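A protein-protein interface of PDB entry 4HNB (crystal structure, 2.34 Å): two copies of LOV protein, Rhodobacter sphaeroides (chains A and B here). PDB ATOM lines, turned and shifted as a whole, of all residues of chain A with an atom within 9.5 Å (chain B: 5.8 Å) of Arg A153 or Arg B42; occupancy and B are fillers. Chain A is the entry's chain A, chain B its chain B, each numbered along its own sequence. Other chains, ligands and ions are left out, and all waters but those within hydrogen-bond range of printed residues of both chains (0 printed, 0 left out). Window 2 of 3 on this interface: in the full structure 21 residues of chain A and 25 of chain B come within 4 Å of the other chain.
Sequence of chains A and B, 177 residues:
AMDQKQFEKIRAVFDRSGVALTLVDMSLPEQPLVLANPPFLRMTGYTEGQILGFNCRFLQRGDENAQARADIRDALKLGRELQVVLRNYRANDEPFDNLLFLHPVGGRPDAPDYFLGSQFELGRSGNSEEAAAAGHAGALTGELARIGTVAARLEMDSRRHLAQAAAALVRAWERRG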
ATOM      1  N   THR A 141      27.373   0.456 -20.563  1.00  0.00           N
ATOM      2  CA  THR A 141      26.512   0.244 -21.713  1.00  0.00           C
ATOM      3  C   THR A 141      25.160  -0.285 -21.259  1.00  0.00           C
ATOM      4  O   THR A 141      24.122   0.117 -21.777  1.00  0.00           O
ATOM      5  CB  THR A 141      27.161  -0.726 -22.718  1.00  0.00           C
ATOM      6  OG1 THR A 141      28.395  -0.165 -23.190  1.00  0.00           O
ATOM      7  CG2 THR A 141      26.237  -0.970 -23.892  1.00  0.00           C
ATOM      8  N   ALA A 145      21.724   1.564 -21.917  1.00  0.00           N
ATOM      9  CA  ALA A 145      20.598   0.849 -22.518  1.00  0.00           C
ATOM     10  C   ALA A 145      19.328   1.011 -21.683  1.00  0.00           C
ATOM     11  O   ALA A 145      18.222   0.984 -22.228  1.00  0.00           O
ATOM     12  CB  ALA A 145      20.925  -0.632 -22.679  1.00  0.00           C
ATOM     13  N   GLY A 148      17.970   4.665 -22.082  1.00  0.00           N
ATOM     14  CA  GLY A 148      17.352   4.725 -23.393  1.00  0.00           C
ATOM     15  C   GLY A 148      18.294   5.195 -24.492  1.00  0.00           C
ATOM     16  O   GLY A 148      17.982   5.063 -25.676  1.00  0.00           O
ATOM     17  N   VAL A 150      21.477   4.146 -25.526  1.00  0.00           N
ATOM     18  CA  VAL A 150      21.818   3.016 -26.387  1.00  0.00           C
ATOM     19  C   VAL A 150      20.540   2.223 -26.711  1.00  0.00           C
ATOM     20  O   VAL A 150      19.919   1.622 -25.832  1.00  0.00           O
ATOM     21  CB  VAL A 150      22.931   2.128 -25.764  1.00  0.00           C
ATOM     22  CG1 VAL A 150      22.879   0.710 -26.319  1.00  0.00           C
ATOM     23  CG2 VAL A 150      24.312   2.762 -25.987  1.00  0.00           C
ATOM     24  N   ALA A 151      20.140   2.258 -27.978  1.00  0.00           N
ATOM     25  CA  ALA A 151      18.872   1.676 -28.408  1.00  0.00           C
ATOM     26  C   ALA A 151      18.867   0.152 -28.325  1.00  0.00           C
ATOM     27  O   ALA A 151      19.913  -0.480 -28.463  1.00  0.00           O
ATOM     28  CB  ALA A 151      18.546   2.123 -29.832  1.00  0.00           C
ATOM     29  N   ALA A 152      17.685  -0.415 -28.082  1.00  0.00           N
ATOM     30  CA  ALA A 152      17.412  -1.847 -28.267  1.00  0.00           C
ATOM     31  C   ALA A 152      18.472  -2.788 -27.704  1.00  0.00           C
ATOM     32  O   ALA A 152      18.956  -2.601 -26.591  1.00  0.00           O
ATOM     33  CB  ALA A 152      17.186  -2.144 -29.744  1.00  0.00           C
ATOM     34  N   ARG A 153      18.815  -3.815 -28.475  1.00  0.00           N
ATOM     35  CA  ARG A 153      19.976  -4.625 -28.126  1.00  0.00           C
ATOM     36  C   ARG A 153      21.000  -4.766 -29.256  1.00  0.00           C
ATOM     37  O   ARG A 153      21.626  -5.813 -29.433  1.00  0.00           O
ATOM     38  CB  ARG A 153      19.607  -5.965 -27.480  1.00  0.00           C
ATOM     39  CG  ARG A 153      18.979  -6.999 -28.377  1.00  0.00           C
ATOM     40  CD  ARG A 153      18.955  -8.303 -27.620  1.00  0.00           C
ATOM     41  NE  ARG A 153      17.995  -9.249 -28.164  1.00  0.00           N
ATOM     42  CZ  ARG A 153      18.333 -10.401 -28.726  1.00  0.00           C
ATOM     43  NH1 ARG A 153      19.611 -10.740 -28.816  1.00  0.00           N
ATOM     44  NH2 ARG A 153      17.398 -11.208 -29.201  1.00  0.00           N
ATOM     45  N   LEU A 154      21.181  -3.671 -29.993  1.00  0.00           N
ATOM     46  CA  LEU A 154      22.462  -3.400 -30.637  1.00  0.00           C
ATOM     47  C   LEU A 154      23.417  -2.921 -29.528  1.00  0.00           C
ATOM     48  O   LEU A 154      24.514  -2.421 -29.787  1.00  0.00           O
ATOM     49  CB  LEU A 154      22.325  -2.366 -31.770  1.00  0.00           C
ATOM     50  CG  LEU A 154      21.665  -0.984 -31.610  1.00  0.00           C
ATOM     51  CD1 LEU A 154      22.390  -0.076 -30.634  1.00  0.00           C
ATOM     52  CD2 LEU A 154      21.575  -0.301 -32.965  1.00  0.00           C
ATOM     53  N   GLU A 155      22.933  -3.047 -28.294  1.00  0.00           N
ATOM     54  CA  GLU A 155      23.687  -2.858 -27.066  1.00  0.00           C
ATOM     55  C   GLU A 155      24.946  -3.721 -27.058  1.00  0.00           C
ATOM     56  O   GLU A 155      26.011  -3.262 -26.647  1.00  0.00           O
ATOM     57  CB  GLU A 155      22.792  -3.215 -25.871  1.00  0.00           C
ATOM     58  CG  GLU A 155      23.515  -3.290 -24.537  1.00  0.00           C
ATOM     59  CD  GLU A 155      22.601  -3.673 -23.382  1.00  0.00           C
ATOM     60  OE1 GLU A 155      21.412  -3.961 -23.629  1.00  0.00           O
ATOM     61  OE2 GLU A 155      23.074  -3.686 -22.224  1.00  0.00           O
ATOM     62  N   MET A 156      24.812  -4.964 -27.525  1.00  0.00           N
ATOM     63  CA  MET A 156      25.921  -5.922 -27.600  1.00  0.00           C
ATOM     64  C   MET A 156      27.116  -5.379 -28.391  1.00  0.00           C
ATOM     65  O   MET A 156      28.250  -5.355 -27.894  1.00  0.00           O
ATOM     66  CB  MET A 156      25.441  -7.257 -28.206  1.00  0.00           C
ATOM     67  CG  MET A 156      26.548  -8.300 -28.368  1.00  0.00           C
ATOM     68  SD  MET A 156      25.974  -9.970 -28.790  1.00  0.00           S
ATOM     69  CE  MET A 156      26.521 -10.109 -30.491  1.00  0.00           C
ATOM     70  N   ASP A 157      26.854  -4.948 -29.624  1.00  0.00           N
ATOM     71  CA  ASP A 157      27.892  -4.374 -30.471  1.00  0.00           C
ATOM     72  C   ASP A 157      28.343  -3.044 -29.897  1.00  0.00           C
ATOM     73  O   ASP A 157      29.529  -2.723 -29.905  1.00  0.00           O
ATOM     74  CB  ASP A 157      27.388  -4.190 -31.899  1.00  0.00           C
ATOM     75  CG  ASP A 157      26.989  -5.502 -32.546  1.00  0.00           C
ATOM     76  OD1 ASP A 157      27.630  -6.535 -32.241  1.00  0.00           O
ATOM     77  OD2 ASP A 157      26.034  -5.497 -33.356  1.00  0.00           O
ATOM     78  N   SER A 158      27.387  -2.269 -29.398  1.00  0.00           N
ATOM     79  CA  SER A 158      27.717  -1.060 -28.657  1.00  0.00           C
ATOM     80  C   SER A 158      28.643  -1.373 -27.476  1.00  0.00           C
ATOM     81  O   SER A 158      29.627  -0.673 -27.270  1.00  0.00           O
ATOM     82  CB  SER A 158      26.459  -0.353 -28.167  1.00  0.00           C
ATOM     83  OG  SER A 158      26.816   0.811 -27.457  1.00  0.00           O
ATOM     84  N   ARG A 159      28.340  -2.434 -26.727  1.00  0.00           N
ATOM     85  CA  ARG A 159      29.188  -2.852 -25.612  1.00  0.00           C
ATOM     86  C   ARG A 159      30.598  -3.220 -26.072  1.00  0.00           C
ATOM     87  O   ARG A 159      31.590  -2.735 -25.511  1.00  0.00           O
ATOM     88  CB  ARG A 159      28.569  -4.026 -24.844  1.00  0.00           C
ATOM     89  CG  ARG A 159      29.480  -4.570 -23.743  1.00  0.00           C
ATOM     90  CD  ARG A 159      28.828  -5.666 -22.921  1.00  0.00           C
ATOM     91  NE  ARG A 159      28.401  -6.813 -23.726  1.00  0.00           N
ATOM     92  CZ  ARG A 159      27.144  -7.044 -24.088  1.00  0.00           C
ATOM     93  NH1 ARG A 159      26.846  -8.115 -24.822  1.00  0.00           N
ATOM     94  NH2 ARG A 159      26.182  -6.201 -23.725  1.00  0.00           N
ATOM     95  N   ARG A 160      30.678  -4.068 -27.098  1.00  0.00           N
ATOM     96  CA  ARG A 160      31.952  -4.566 -27.616  1.00  0.00           C
ATOM     97  C   ARG A 160      32.865  -3.450 -28.095  1.00  0.00           C
ATOM     98  O   ARG A 160      34.069  -3.475 -27.840  1.00  0.00           O
ATOM     99  CB  ARG A 160      31.714  -5.562 -28.757  1.00  0.00           C
ATOM    100  CG  ARG A 160      32.990  -6.074 -29.412  1.00  0.00           C
ATOM    101  CD  ARG A 160      32.876  -7.557 -29.700  1.00  0.00           C
ATOM    102  NE  ARG A 160      31.767  -7.839 -30.612  1.00  0.00           N
ATOM    103  CZ  ARG A 160      31.008  -8.928 -30.560  1.00  0.00           C
ATOM    104  NH1 ARG A 160      30.022  -9.089 -31.433  1.00  0.00           N
ATOM    105  NH2 ARG A 160      31.230  -9.852 -29.631  1.00  0.00           N
ATOM    106  N   SER B  17      17.764  -7.937 -20.898  1.00  0.00           N
ATOM    107  CA  SER B  17      19.225  -7.952 -20.890  1.00  0.00           C
ATOM    108  C   SER B  17      19.880  -7.976 -22.269  1.00  0.00           C
ATOM    109  O   SER B  17      19.342  -8.526 -23.225  1.00  0.00           O
ATOM    110  CB  SER B  17      19.746  -9.133 -20.065  1.00  0.00           C
ATOM    111  OG  SER B  17      21.156  -9.071 -19.890  1.00  0.00           O
ATOM    112  N   GLY B  18      21.070  -7.393 -22.340  1.00  0.00           N
ATOM    113  CA  GLY B  18      21.871  -7.408 -23.546  1.00  0.00           C
ATOM    114  C   GLY B  18      22.898  -8.531 -23.559  1.00  0.00           C
ATOM    115  O   GLY B  18      23.726  -8.596 -24.468  1.00  0.00           O
ATOM    116  N   ASN B  37      16.864 -16.226 -22.173  1.00  0.00           N
ATOM    117  CA  ASN B  37      16.484 -14.952 -22.781  1.00  0.00           C
ATOM    118  C   ASN B  37      16.763 -14.887 -24.294  1.00  0.00           C
ATOM    119  O   ASN B  37      17.387 -15.805 -24.845  1.00  0.00           O
ATOM    120  CB  ASN B  37      17.095 -13.775 -21.991  1.00  0.00           C
ATOM    121  CG  ASN B  37      18.573 -13.619 -22.228  1.00  0.00           C
ATOM    122  OD1 ASN B  37      19.200 -14.443 -22.896  1.00  0.00           O
ATOM    123  ND2 ASN B  37      19.145 -12.559 -21.680  1.00  0.00           N
ATOM    124  N   PRO B  38      16.265 -13.832 -24.979  1.00  0.00           N
ATOM    125  CA  PRO B  38      16.455 -13.747 -26.436  1.00  0.00           C
ATOM    126  C   PRO B  38      17.896 -13.875 -26.973  1.00  0.00           C
ATOM    127  O   PRO B  38      18.079 -14.599 -27.951  1.00  0.00           O
ATOM    128  CB  PRO B  38      15.826 -12.394 -26.784  1.00  0.00           C
ATOM    129  CG  PRO B  38      14.728 -12.245 -25.788  1.00  0.00           C
ATOM    130  CD  PRO B  38      15.246 -12.869 -24.517  1.00  0.00           C
ATOM    131  N   PRO B  39      18.887 -13.201 -26.362  1.00  0.00           N
ATOM    132  CA  PRO B  39      20.249 -13.362 -26.890  1.00  0.00           C
ATOM    133  C   PRO B  39      20.817 -14.784 -26.748  1.00  0.00           C
ATOM    134  O   PRO B  39      21.682 -15.163 -27.536  1.00  0.00           O
ATOM    135  CB  PRO B  39      21.071 -12.356 -26.055  1.00  0.00           C
ATOM    136  CG  PRO B  39      20.046 -11.351 -25.532  1.00  0.00           C
ATOM    137  CD  PRO B  39      18.825 -12.179 -25.296  1.00  0.00           C
ATOM    138  N   PHE B  40      20.377 -15.564 -25.764  1.00  0.00           N
ATOM    139  CA  PHE B  40      20.849 -16.945 -25.670  1.00  0.00           C
ATOM    140  C   PHE B  40      20.180 -17.715 -26.812  1.00  0.00           C
ATOM    141  O   PHE B  40      20.780 -18.581 -27.456  1.00  0.00           O
ATOM    142  CB  PHE B  40      20.494 -17.559 -24.310  1.00  0.00           C
ATOM    143  CG  PHE B  40      20.672 -19.071 -24.246  1.00  0.00           C
ATOM    144  CD1 PHE B  40      21.915 -19.634 -23.975  1.00  0.00           C
ATOM    145  CD2 PHE B  40      19.595 -19.928 -24.460  1.00  0.00           C
ATOM    146  CE1 PHE B  40      22.080 -21.022 -23.923  1.00  0.00           C
ATOM    147  CE2 PHE B  40      19.760 -21.323 -24.408  1.00  0.00           C
ATOM    148  CZ  PHE B  40      21.002 -21.866 -24.144  1.00  0.00           C
ATOM    149  N   LEU B  41      18.923 -17.376 -27.061  1.00  0.00           N
ATOM    150  CA  LEU B  41      18.136 -18.071 -28.062  1.00  0.00           C
ATOM    151  C   LEU B  41      18.641 -17.807 -29.483  1.00  0.00           C
ATOM    152  O   LEU B  41      18.639 -18.719 -30.312  1.00  0.00           O
ATOM    153  CB  LEU B  41      16.650 -17.745 -27.899  1.00  0.00           C
ATOM    154  CG  LEU B  41      16.074 -18.281 -26.574  1.00  0.00           C
ATOM    155  CD1 LEU B  41      14.630 -17.843 -26.353  1.00  0.00           C
ATOM    156  CD2 LEU B  41      16.195 -19.811 -26.470  1.00  0.00           C
ATOM    157  N   ARG B  42      19.115 -16.593 -29.757  1.00  0.00           N
ATOM    158  CA  ARG B  42      19.698 -16.289 -31.078  1.00  0.00           C
ATOM    159  C   ARG B  42      21.061 -16.932 -31.272  1.00  0.00           C
ATOM    160  O   ARG B  42      21.346 -17.479 -32.336  1.00  0.00           O
ATOM    161  CB  ARG B  42      19.857 -14.787 -31.306  1.00  0.00           C
ATOM    162  CG  ARG B  42      18.579 -14.039 -31.541  1.00  0.00           C
ATOM    163  CD  ARG B  42      18.844 -12.547 -31.578  1.00  0.00           C
ATOM    164  NE  ARG B  42      19.380 -12.118 -32.859  1.00  0.00           N
ATOM    165  CZ  ARG B  42      18.623 -11.768 -33.894  1.00  0.00           C
ATOM    166  NH1 ARG B  42      17.301 -11.800 -33.793  1.00  0.00           N
ATOM    167  NH2 ARG B  42      19.189 -11.390 -35.031  1.00  0.00           N
ATOM    168  N   MET B  43      21.912 -16.827 -30.252  1.00  0.00           N
ATOM    169  CA  MET B  43      23.241 -17.427 -30.309  1.00  0.00           C
ATOM    170  C   MET B  43      23.133 -18.904 -30.689  1.00  0.00           C
ATOM    171  O   MET B  43      23.891 -19.390 -31.526  1.00  0.00           O
ATOM    172  CB  MET B  43      23.953 -17.270 -28.967  1.00  0.00           C
ATOM    173  CG  MET B  43      25.323 -17.904 -28.899  1.00  0.00           C
ATOM    174  SD  MET B  43      26.014 -17.743 -27.233  1.00  0.00           S
ATOM    175  CE  MET B  43      25.038 -18.983 -26.409  1.00  0.00           C
ATOM    176  N   THR B  44      22.163 -19.595 -30.091  1.00  0.00           N
ATOM    177  CA  THR B  44      22.011 -21.044 -30.273  1.00  0.00           C
ATOM    178  C   THR B  44      21.072 -21.430 -31.415  1.00  0.00           C
ATOM    179  O   THR B  44      21.211 -22.505 -32.000  1.00  0.00           O
ATOM    180  CB  THR B  44      21.504 -21.724 -28.992  1.00  0.00           C
ATOM    181  OG1 THR B  44      20.225 -21.172 -28.640  1.00  0.00           O
ATOM    182  CG2 THR B  44      22.488 -21.511 -27.849  1.00  0.00           C
ATOM    183  N   GLY B  45      20.103 -20.571 -31.716  1.00  0.00           N
ATOM    184  CA  GLY B  45      19.184 -20.834 -32.808  1.00  0.00           C
ATOM    185  C   GLY B  45      17.974 -21.683 -32.445  1.00  0.00           C
ATOM    186  O   GLY B  45      17.325 -22.261 -33.322  1.00  0.00           O
ATOM    187  N   TYR B  46      17.652 -21.759 -31.158  1.00  0.00           N
ATOM    188  CA  TYR B  46      16.445 -22.450 -30.725  1.00  0.00           C
ATOM    189  C   TYR B  46      15.339 -21.432 -30.424  1.00  0.00           C
ATOM    190  O   TYR B  46      15.550 -20.235 -30.580  1.00  0.00           O
ATOM    191  CB  TYR B  46      16.747 -23.345 -29.521  1.00  0.00           C
ATOM    192  CG  TYR B  46      17.718 -24.456 -29.842  1.00  0.00           C
ATOM    193  CD1 TYR B  46      19.086 -24.239 -29.774  1.00  0.00           C
ATOM    194  CD2 TYR B  46      17.273 -25.714 -30.233  1.00  0.00           C
ATOM    195  CE1 TYR B  46      19.984 -25.231 -30.079  1.00  0.00           C
ATOM    196  CE2 TYR B  46      18.180 -26.731 -30.545  1.00  0.00           C
ATOM    197  CZ  TYR B  46      19.534 -26.471 -30.462  1.00  0.00           C
ATOM    198  OH  TYR B  46      20.471 -27.433 -30.755  1.00  0.00           O
ATOM    199  N   ARG B  90      25.286 -24.915 -32.221  1.00  0.00           N
ATOM    200  CA  ARG B  90      24.004 -24.313 -32.563  1.00  0.00           C
ATOM    201  C   ARG B  90      23.033 -25.360 -33.096  1.00  0.00           C
ATOM    202  O   ARG B  90      23.418 -26.505 -33.355  1.00  0.00           O
ATOM    203  CB  ARG B  90      24.193 -23.245 -33.634  1.00  0.00           C
ATOM    204  CG  ARG B  90      25.268 -22.247 -33.323  1.00  0.00           C
ATOM    205  CD  ARG B  90      25.336 -21.158 -34.378  1.00  0.00           C
ATOM    206  NE  ARG B  90      26.709 -20.689 -34.529  1.00  0.00           N
ATOM    207  CZ  ARG B  90      27.208 -19.614 -33.932  1.00  0.00           C
ATOM    208  NH1 ARG B  90      28.478 -19.274 -34.149  1.00  0.00           N
ATOM    209  NH2 ARG B  90      26.441 -18.879 -33.123  1.00  0.00           N
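The backbone carbonyl oxygen of Gly B18 lies within hydrogen-bond range of the guanidinium group of Arg A159.
Among the printed residues, pairs that only touch across the chains: Arg A153 with Arg B42, Arg A153 with Pro B38, Arg A153 with Pro B39 and Glu A155 with Gly B18.
Arg A153 touches just these residues of chain B: Pro B38 (3.1 Å), Pro B39 (3.3 Å) and Arg B42 (3.1 Å).
Of chain A, only Arg A153 comes within 4 Å of Arg B42.
Pro B39 touches just one residue of chain A: Arg A153.
Printed residues of chain A within 4 Å of Gly B18: Glu A155 (3.5 Å) and Arg A159 (3.2 Å).
Printed residues of chain B within 4 Å of Glu A155: Gly B18 (3.5 Å).
Arg A160 touches none of the printed residues of chain B.
The nearest residue of chain A that does not touch Arg B42 is Met A156 (7.8 Å).
Of the 14 printed residues of chain A, 3 touch a printed residue of chain B.
Hydrophobic or aromatic side chains of chain B within 4 Å of the printed part of chain A: Pro B38 and Pro B39.
Along chain B the printed residues that touch a printed residue of chain A span positions 18 to 42.
No position is printed for both chains.
Of the 5 pairs that touch across the chains among the printed residues, none has its exchanged pair printed and touching as well.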
